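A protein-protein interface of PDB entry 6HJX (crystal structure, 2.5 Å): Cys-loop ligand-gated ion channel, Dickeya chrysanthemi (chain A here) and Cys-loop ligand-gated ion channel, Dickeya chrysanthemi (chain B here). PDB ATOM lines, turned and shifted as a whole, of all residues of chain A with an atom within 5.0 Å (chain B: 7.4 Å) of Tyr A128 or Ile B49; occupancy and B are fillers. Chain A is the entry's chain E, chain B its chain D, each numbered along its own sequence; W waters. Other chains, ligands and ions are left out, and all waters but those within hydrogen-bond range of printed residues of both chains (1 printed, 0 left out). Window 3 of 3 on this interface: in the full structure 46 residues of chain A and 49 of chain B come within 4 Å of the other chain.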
ATOM      1  N   TRP A  65      10.322 -26.054  26.412  1.00  0.00           N
ATOM      2  CA  TRP A  65       9.887 -26.475  25.086  1.00  0.00           C
ATOM      3  C   TRP A  65      10.997 -27.287  24.428  1.00  0.00           C
ATOM      4  O   TRP A  65      12.110 -26.787  24.237  1.00  0.00           O
ATOM      5  CB  TRP A  65       9.526 -25.257  24.236  1.00  0.00           C
ATOM      6  CG  TRP A  65       9.023 -25.578  22.859  1.00  0.00           C
ATOM      7  CD1 TRP A  65       7.816 -26.126  22.534  1.00  0.00           C
ATOM      8  CD2 TRP A  65       9.705 -25.346  21.618  1.00  0.00           C
ATOM      9  NE1 TRP A  65       7.707 -26.258  21.170  1.00  0.00           N
ATOM     10  CE2 TRP A  65       8.853 -25.786  20.585  1.00  0.00           C
ATOM     11  CE3 TRP A  65      10.953 -24.814  21.281  1.00  0.00           C
ATOM     12  CZ2 TRP A  65       9.209 -25.712  19.239  1.00  0.00           C
ATOM     13  CZ3 TRP A  65      11.306 -24.742  19.942  1.00  0.00           C
ATOM     14  CH2 TRP A  65      10.437 -25.188  18.939  1.00  0.00           C
ATOM     15  N   PRO A  67      10.960 -29.590  21.069  1.00  0.00           N
ATOM     16  CA  PRO A  67      10.170 -30.187  19.989  1.00  0.00           C
ATOM     17  C   PRO A  67      10.695 -31.558  19.598  1.00  0.00           C
ATOM     18  O   PRO A  67      11.901 -31.814  19.620  1.00  0.00           O
ATOM     19  CB  PRO A  67      10.319 -29.180  18.843  1.00  0.00           C
ATOM     20  CG  PRO A  67      11.635 -28.528  19.101  1.00  0.00           C
ATOM     21  CD  PRO A  67      11.763 -28.447  20.597  1.00  0.00           C
ATOM     22  N   PRO A 125      10.427 -32.098  11.721  1.00  0.00           N
ATOM     23  CA  PRO A 125       9.649 -31.999  12.958  1.00  0.00           C
ATOM     24  C   PRO A 125       8.351 -32.781  12.836  1.00  0.00           C
ATOM     25  O   PRO A 125       7.772 -32.902  11.754  1.00  0.00           O
ATOM     26  CB  PRO A 125       9.391 -30.495  13.106  1.00  0.00           C
ATOM     27  CG  PRO A 125      10.397 -29.834  12.235  1.00  0.00           C
ATOM     28  CD  PRO A 125      10.647 -30.776  11.106  1.00  0.00           C
ATOM     29  N   PHE A 126       7.896 -33.320  13.968  1.00  0.00           N
ATOM     30  CA  PHE A 126       6.719 -34.179  13.978  1.00  0.00           C
ATOM     31  C   PHE A 126       5.416 -33.397  14.065  1.00  0.00           C
ATOM     32  O   PHE A 126       4.378 -33.901  13.624  1.00  0.00           O
ATOM     33  CB  PHE A 126       6.803 -35.163  15.152  1.00  0.00           C
ATOM     34  CG  PHE A 126       5.741 -36.227  15.128  1.00  0.00           C
ATOM     35  CD1 PHE A 126       5.873 -37.331  14.304  1.00  0.00           C
ATOM     36  CD2 PHE A 126       4.614 -36.124  15.926  1.00  0.00           C
ATOM     37  CE1 PHE A 126       4.899 -38.314  14.272  1.00  0.00           C
ATOM     38  CE2 PHE A 126       3.635 -37.105  15.900  1.00  0.00           C
ATOM     39  CZ  PHE A 126       3.780 -38.200  15.071  1.00  0.00           C
ATOM     40  N   SER A 127       5.443 -32.181  14.608  1.00  0.00           N
ATOM     41  CA  SER A 127       4.220 -31.442  14.897  1.00  0.00           C
ATOM     42  C   SER A 127       4.242 -29.980  14.482  1.00  0.00           C
ATOM     43  O   SER A 127       3.164 -29.410  14.272  1.00  0.00           O
ATOM     44  CB  SER A 127       3.906 -31.500  16.402  1.00  0.00           C
ATOM     45  OG  SER A 127       3.975 -32.827  16.898  1.00  0.00           O
ATOM     46  N   TYR A 128       5.407 -29.350  14.360  1.00  0.00           N
ATOM     47  CA  TYR A 128       5.493 -27.911  14.147  1.00  0.00           C
ATOM     48  C   TYR A 128       5.831 -27.623  12.690  1.00  0.00           C
ATOM     49  O   TYR A 128       6.869 -28.067  12.185  1.00  0.00           O
ATOM     50  CB  TYR A 128       6.525 -27.294  15.088  1.00  0.00           C
ATOM     51  CG  TYR A 128       6.157 -27.475  16.541  1.00  0.00           C
ATOM     52  CD1 TYR A 128       5.240 -26.632  17.154  1.00  0.00           C
ATOM     53  CD2 TYR A 128       6.707 -28.500  17.294  1.00  0.00           C
ATOM     54  CE1 TYR A 128       4.889 -26.799  18.479  1.00  0.00           C
ATOM     55  CE2 TYR A 128       6.365 -28.675  18.623  1.00  0.00           C
ATOM     56  CZ  TYR A 128       5.453 -27.822  19.209  1.00  0.00           C
ATOM     57  OH  TYR A 128       5.107 -27.990  20.530  1.00  0.00           O
ATOM     58  N   ASN A 129       4.944 -26.891  12.018  1.00  0.00           N
ATOM     59  CA  ASN A 129       5.155 -26.489  10.638  1.00  0.00           C
ATOM     60  C   ASN A 129       6.293 -25.471  10.558  1.00  0.00           C
ATOM     61  O   ASN A 129       6.856 -25.040  11.570  1.00  0.00           O
ATOM     62  CB  ASN A 129       3.864 -25.919  10.051  1.00  0.00           C
ATOM     63  CG  ASN A 129       3.246 -24.852  10.930  1.00  0.00           C
ATOM     64  OD1 ASN A 129       3.711 -23.715  10.964  1.00  0.00           O
ATOM     65  ND2 ASN A 129       2.190 -25.215  11.646  1.00  0.00           N
ATOM     66  N   ASN A 130       6.636 -25.077   9.332  1.00  0.00           N
ATOM     67  CA  ASN A 130       7.754 -24.165   9.119  1.00  0.00           C
ATOM     68  C   ASN A 130       7.388 -22.704   9.367  1.00  0.00           C
ATOM     69  O   ASN A 130       8.198 -21.820   9.065  1.00  0.00           O
ATOM     70  CB  ASN A 130       8.318 -24.335   7.707  1.00  0.00           C
ATOM     71  CG  ASN A 130       7.324 -23.984   6.629  1.00  0.00           C
ATOM     72  OD1 ASN A 130       6.222 -23.515   6.905  1.00  0.00           O
ATOM     73  ND2 ASN A 130       7.720 -24.199   5.380  1.00  0.00           N
ATOM     74  N   GLN A 132       6.396 -22.221  12.584  1.00  0.00           N
ATOM     75  CA  GLN A 132       6.760 -22.301  13.988  1.00  0.00           C
ATOM     76  C   GLN A 132       8.182 -22.793  14.213  1.00  0.00           C
ATOM     77  O   GLN A 132       8.768 -22.479  15.255  1.00  0.00           O
ATOM     78  CB  GLN A 132       5.792 -23.237  14.729  1.00  0.00           C
ATOM     79  CG  GLN A 132       4.321 -22.898  14.537  1.00  0.00           C
ATOM     80  CD  GLN A 132       3.401 -24.005  15.017  1.00  0.00           C
ATOM     81  OE1 GLN A 132       3.376 -25.099  14.448  1.00  0.00           O
ATOM     82  NE2 GLN A 132       2.637 -23.728  16.071  1.00  0.00           N
ATOM     83  N   LEU A 133       8.751 -23.539  13.267  1.00  0.00           N
ATOM     84  CA  LEU A 133      10.059 -24.163  13.451  1.00  0.00           C
ATOM     85  C   LEU A 133      10.620 -24.502  12.081  1.00  0.00           C
ATOM     86  O   LEU A 133      10.007 -25.279  11.342  1.00  0.00           O
ATOM     87  CB  LEU A 133       9.939 -25.424  14.312  1.00  0.00           C
ATOM     88  CG  LEU A 133      11.205 -26.066  14.886  1.00  0.00           C
ATOM     89  CD1 LEU A 133      10.812 -27.133  15.900  1.00  0.00           C
ATOM     90  CD2 LEU A 133      12.081 -26.680  13.810  1.00  0.00           C
ATOM     91  N   PHE A 181       6.213 -28.190   6.150  1.00  0.00           N
ATOM     92  CA  PHE A 181       7.179 -28.628   7.146  1.00  0.00           C
ATOM     93  C   PHE A 181       8.583 -28.580   6.560  1.00  0.00           C
ATOM     94  O   PHE A 181       8.789 -28.886   5.382  1.00  0.00           O
ATOM     95  CB  PHE A 181       6.861 -30.048   7.644  1.00  0.00           C
ATOM     96  CG  PHE A 181       5.729 -30.106   8.631  1.00  0.00           C
ATOM     97  CD1 PHE A 181       4.412 -30.063   8.202  1.00  0.00           C
ATOM     98  CD2 PHE A 181       5.982 -30.212   9.987  1.00  0.00           C
ATOM     99  CE1 PHE A 181       3.369 -30.116   9.110  1.00  0.00           C
ATOM    100  CE2 PHE A 181       4.943 -30.268  10.900  1.00  0.00           C
ATOM    101  CZ  PHE A 181       3.636 -30.219  10.459  1.00  0.00           C
ATOM    102  N   PRO B  43      -3.734 -21.500  25.091  1.00  0.00           N
ATOM    103  CA  PRO B  43      -2.848 -20.331  25.077  1.00  0.00           C
ATOM    104  C   PRO B  43      -3.083 -19.475  23.842  1.00  0.00           C
ATOM    105  O   PRO B  43      -3.088 -19.972  22.712  1.00  0.00           O
ATOM    106  CB  PRO B  43      -1.446 -20.949  25.080  1.00  0.00           C
ATOM    107  CG  PRO B  43      -1.624 -22.293  25.691  1.00  0.00           C
ATOM    108  CD  PRO B  43      -2.983 -22.759  25.258  1.00  0.00           C
ATOM    109  N   LYS B  46      -5.208 -20.230  20.520  1.00  0.00           N
ATOM    110  CA  LYS B  46      -4.659 -20.884  19.343  1.00  0.00           C
ATOM    111  C   LYS B  46      -4.558 -22.386  19.579  1.00  0.00           C
ATOM    112  O   LYS B  46      -4.625 -22.850  20.725  1.00  0.00           O
ATOM    113  CB  LYS B  46      -3.274 -20.319  18.999  1.00  0.00           C
ATOM    114  N   PRO B  47      -4.402 -23.179  18.519  1.00  0.00           N
ATOM    115  CA  PRO B  47      -4.299 -24.632  18.703  1.00  0.00           C
ATOM    116  C   PRO B  47      -3.113 -24.997  19.584  1.00  0.00           C
ATOM    117  O   PRO B  47      -2.044 -24.389  19.502  1.00  0.00           O
ATOM    118  CB  PRO B  47      -4.129 -25.163  17.274  1.00  0.00           C
ATOM    119  CG  PRO B  47      -4.679 -24.097  16.399  1.00  0.00           C
ATOM    120  CD  PRO B  47      -4.390 -22.802  17.095  1.00  0.00           C
ATOM    121  N   LEU B  48      -3.315 -25.999  20.435  1.00  0.00           N
ATOM    122  CA  LEU B  48      -2.308 -26.446  21.387  1.00  0.00           C
ATOM    123  C   LEU B  48      -1.795 -27.822  20.986  1.00  0.00           C
ATOM    124  O   LEU B  48      -2.583 -28.749  20.774  1.00  0.00           O
ATOM    125  CB  LEU B  48      -2.880 -26.490  22.806  1.00  0.00           C
ATOM    126  CG  LEU B  48      -1.947 -27.025  23.895  1.00  0.00           C
ATOM    127  CD1 LEU B  48      -0.622 -26.272  23.911  1.00  0.00           C
ATOM    128  CD2 LEU B  48      -2.619 -26.944  25.254  1.00  0.00           C
ATOM    129  N   ILE B  49      -0.475 -27.949  20.886  1.00  0.00           N
ATOM    130  CA  ILE B  49       0.178 -29.201  20.529  1.00  0.00           C
ATOM    131  C   ILE B  49       0.712 -29.841  21.801  1.00  0.00           C
ATOM    132  O   ILE B  49       1.341 -29.168  22.629  1.00  0.00           O
ATOM    133  CB  ILE B  49       1.304 -28.968  19.505  1.00  0.00           C
ATOM    134  CG1 ILE B  49       0.702 -28.640  18.135  1.00  0.00           C
ATOM    135  CG2 ILE B  49       2.216 -30.188  19.414  1.00  0.00           C
ATOM    136  CD1 ILE B  49       1.709 -28.142  17.112  1.00  0.00           C
ATOM    137  N   VAL B  50       0.455 -31.137  21.963  1.00  0.00           N
ATOM    138  CA  VAL B  50       0.908 -31.901  23.121  1.00  0.00           C
ATOM    139  C   VAL B  50       1.536 -33.187  22.603  1.00  0.00           C
ATOM    140  O   VAL B  50       0.883 -33.951  21.882  1.00  0.00           O
ATOM    141  CB  VAL B  50      -0.240 -32.212  24.094  1.00  0.00           C
ATOM    142  CG1 VAL B  50       0.314 -32.742  25.403  1.00  0.00           C
ATOM    143  CG2 VAL B  50      -1.097 -30.974  24.327  1.00  0.00           C
ATOM    144  N   GLU B  51       2.789 -33.433  22.979  1.00  0.00           N
ATOM    145  CA  GLU B  51       3.594 -34.481  22.370  1.00  0.00           C
ATOM    146  C   GLU B  51       3.957 -35.563  23.376  1.00  0.00           C
ATOM    147  O   GLU B  51       4.284 -35.271  24.531  1.00  0.00           O
ATOM    148  CB  GLU B  51       4.882 -33.900  21.773  1.00  0.00           C
ATOM    149  CG  GLU B  51       4.675 -33.084  20.517  1.00  0.00           C
ATOM    150  CD  GLU B  51       5.984 -32.683  19.875  1.00  0.00           C
ATOM    151  OE1 GLU B  51       6.932 -32.348  20.616  1.00  0.00           O
ATOM    152  OE2 GLU B  51       6.069 -32.718  18.630  1.00  0.00           O
ATOM    153  N   GLN B  54       3.769 -36.028  27.423  1.00  0.00           N
ATOM    154  CA  GLN B  54       2.844 -35.040  27.964  1.00  0.00           C
ATOM    155  C   GLN B  54       1.384 -35.404  27.714  1.00  0.00           C
ATOM    156  O   GLN B  54       0.509 -34.919  28.439  1.00  0.00           O
ATOM    157  CB  GLN B  54       3.156 -33.666  27.374  1.00  0.00           C
ATOM    158  CG  GLN B  54       4.575 -33.206  27.652  1.00  0.00           C
ATOM    159  CD  GLN B  54       4.913 -33.250  29.126  1.00  0.00           C
ATOM    160  OE1 GLN B  54       4.064 -32.979  29.975  1.00  0.00           O
ATOM    161  NE2 GLN B  54       6.150 -33.615  29.441  1.00  0.00           N
ATOM    162  N   TRP B  58      -2.661 -35.015  30.230  1.00  0.00           N
ATOM    163  CA  TRP B  58      -4.007 -34.565  29.891  1.00  0.00           C
ATOM    164  C   TRP B  58      -5.033 -35.670  30.113  1.00  0.00           C
ATOM    165  O   TRP B  58      -6.148 -35.404  30.578  1.00  0.00           O
ATOM    166  CB  TRP B  58      -4.052 -34.080  28.444  1.00  0.00           C
ATOM    167  CG  TRP B  58      -3.446 -32.722  28.243  1.00  0.00           C
ATOM    168  CD1 TRP B  58      -2.120 -32.422  28.146  1.00  0.00           C
ATOM    169  CD2 TRP B  58      -4.149 -31.481  28.109  1.00  0.00           C
ATOM    170  NE1 TRP B  58      -1.951 -31.071  27.964  1.00  0.00           N
ATOM    171  CE2 TRP B  58      -3.182 -30.470  27.937  1.00  0.00           C
ATOM    172  CE3 TRP B  58      -5.501 -31.125  28.120  1.00  0.00           C
ATOM    173  CZ2 TRP B  58      -3.524 -29.129  27.777  1.00  0.00           C
ATOM    174  CZ3 TRP B  58      -5.839 -29.794  27.961  1.00  0.00           C
ATOM    175  CH2 TRP B  58      -4.854 -28.812  27.793  1.00  0.00           C
ATOM    176  N   ARG B  83       1.234 -37.264  18.973  1.00  0.00           N
ATOM    177  CA  ARG B  83       0.860 -35.950  19.468  1.00  0.00           C
ATOM    178  C   ARG B  83      -0.654 -35.802  19.492  1.00  0.00           C
ATOM    179  O   ARG B  83      -1.387 -36.519  18.805  1.00  0.00           O
ATOM    180  CB  ARG B  83       1.463 -34.825  18.610  1.00  0.00           C
ATOM    181  CG  ARG B  83       0.893 -34.739  17.194  1.00  0.00           C
ATOM    182  CD  ARG B  83       0.752 -33.298  16.720  1.00  0.00           C
ATOM    183  NE  ARG B  83      -0.190 -33.184  15.611  1.00  0.00           N
ATOM    184  CZ  ARG B  83       0.097 -33.480  14.346  1.00  0.00           C
ATOM    185  NH1 ARG B  83       1.306 -33.915  14.017  1.00  0.00           N
ATOM    186  NH2 ARG B  83      -0.832 -33.343  13.408  1.00  0.00           N
ATOM    187  N   LEU B  84      -1.107 -34.849  20.296  1.00  0.00           N
ATOM    188  CA  LEU B  84      -2.467 -34.338  20.245  1.00  0.00           C
ATOM    189  C   LEU B  84      -2.433 -32.897  19.752  1.00  0.00           C
ATOM    190  O   LEU B  84      -1.471 -32.165  20.001  1.00  0.00           O
ATOM    191  CB  LEU B  84      -3.140 -34.388  21.619  1.00  0.00           C
ATOM    192  CG  LEU B  84      -3.449 -35.761  22.214  1.00  0.00           C
ATOM    193  CD1 LEU B  84      -3.916 -35.601  23.652  1.00  0.00           C
ATOM    194  CD2 LEU B  84      -4.500 -36.489  21.389  1.00  0.00           C
ATOM    195  N   MET B  85      -3.485 -32.500  19.042  1.00  0.00           N
ATOM    196  CA  MET B  85      -3.693 -31.101  18.678  1.00  0.00           C
ATOM    197  C   MET B  85      -5.082 -30.716  19.164  1.00  0.00           C
ATOM    198  O   MET B  85      -6.087 -31.179  18.612  1.00  0.00           O
ATOM    199  CB  MET B  85      -3.549 -30.881  17.172  1.00  0.00           C
ATOM    200  CG  MET B  85      -3.222 -29.438  16.803  1.00  0.00           C
ATOM    201  SD  MET B  85      -2.998 -29.176  15.033  1.00  0.00           S
ATOM    202  CE  MET B  85      -1.620 -30.272  14.687  1.00  0.00           C
ATOM    203  N   LEU B  86      -5.137 -29.885  20.201  1.00  0.00           N
ATOM    204  CA  LEU B  86      -6.388 -29.536  20.868  1.00  0.00           C
ATOM    205  C   LEU B  86      -6.816 -28.145  20.417  1.00  0.00           C
ATOM    206  O   LEU B  86      -6.149 -27.151  20.723  1.00  0.00           O
ATOM    207  CB  LEU B  86      -6.220 -29.603  22.384  1.00  0.00           C
ATOM    208  CG  LEU B  86      -5.649 -30.921  22.919  1.00  0.00           C
ATOM    209  CD1 LEU B  86      -5.547 -30.878  24.437  1.00  0.00           C
ATOM    210  CD2 LEU B  86      -6.486 -32.118  22.466  1.00  0.00           C
HETATM  211  O   HOH W   1       7.801 -31.535  16.846  1.00  0.00           O
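Glu B51 touches Pro A67.
Ser A127 touches Ile B49.
Ser A127 touches Arg B83 (OG to CD, 3.3 Å).
CD1 of Ile B49 touches CE1 of Tyr A128, 3.7 Å away.
Water W1 lies within hydrogen-bond range of the side-chain carboxylate of Glu B51, the backbone NH of Ser A127 and the backbone NH of Phe A126.
The side-chain hydroxyl (OH) of Tyr A128 sits at hydrogen-bond distance from the indole nitrogen (NE1) of Trp A65, at 3.2 Å.
Of the 13 printed residues of chain B, 3 touch a printed residue of chain A.
Hydrophobic or aromatic side chains of chain B within 4 Å of the printed part of chain A: Ile B49.
Along chain B the printed residues that touch a printed residue of chain A span positions 49 to 83.
Of the 11 printed residues of chain A, 4 touch a printed residue of chain B.
Hydrophobic or aromatic side chains of chain A that line the printed part of chain B: Phe A126 and Tyr A128.
Among the printed residues, 6 pairs touch across the chains.
Among the printed residues, no Asp or Glu carboxylate lies within 4 Å of a Lys or Arg side-chain nitrogen of the other chain.
The side-chain carboxylate (OE2) of Glu B51 sits at hydrogen-bond distance from the side-chain hydroxyl (OG) of Ser A127 (2.7 Å).
The guanidinium group (NH1) of Arg B83 is in hydrogen-bond range of the backbone carbonyl oxygen (O) of Phe A126 (3.1 Å).
Of chain A, only Ser A127 (3.4 Å) and Tyr A128 (3.7 Å) come within 4 Å of Ile B49.
Of the printed residues of chain A, Arg B83 touches Phe A126 and Ser A127.
Of the printed residues of chain B, Pro A67 touches Glu B51.
Printed residues of chain A within 4 Å of Glu B51: Pro A67 and Ser A127.
Lys B46 touches none of the printed residues of chain A.
The nearest residue of chain A that does not touch Ile B49 is Gln A132 (4.4 Å).
The nearest printed residue of chain B that does not touch Pro A67 is Ile B49 (8.0 Å).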
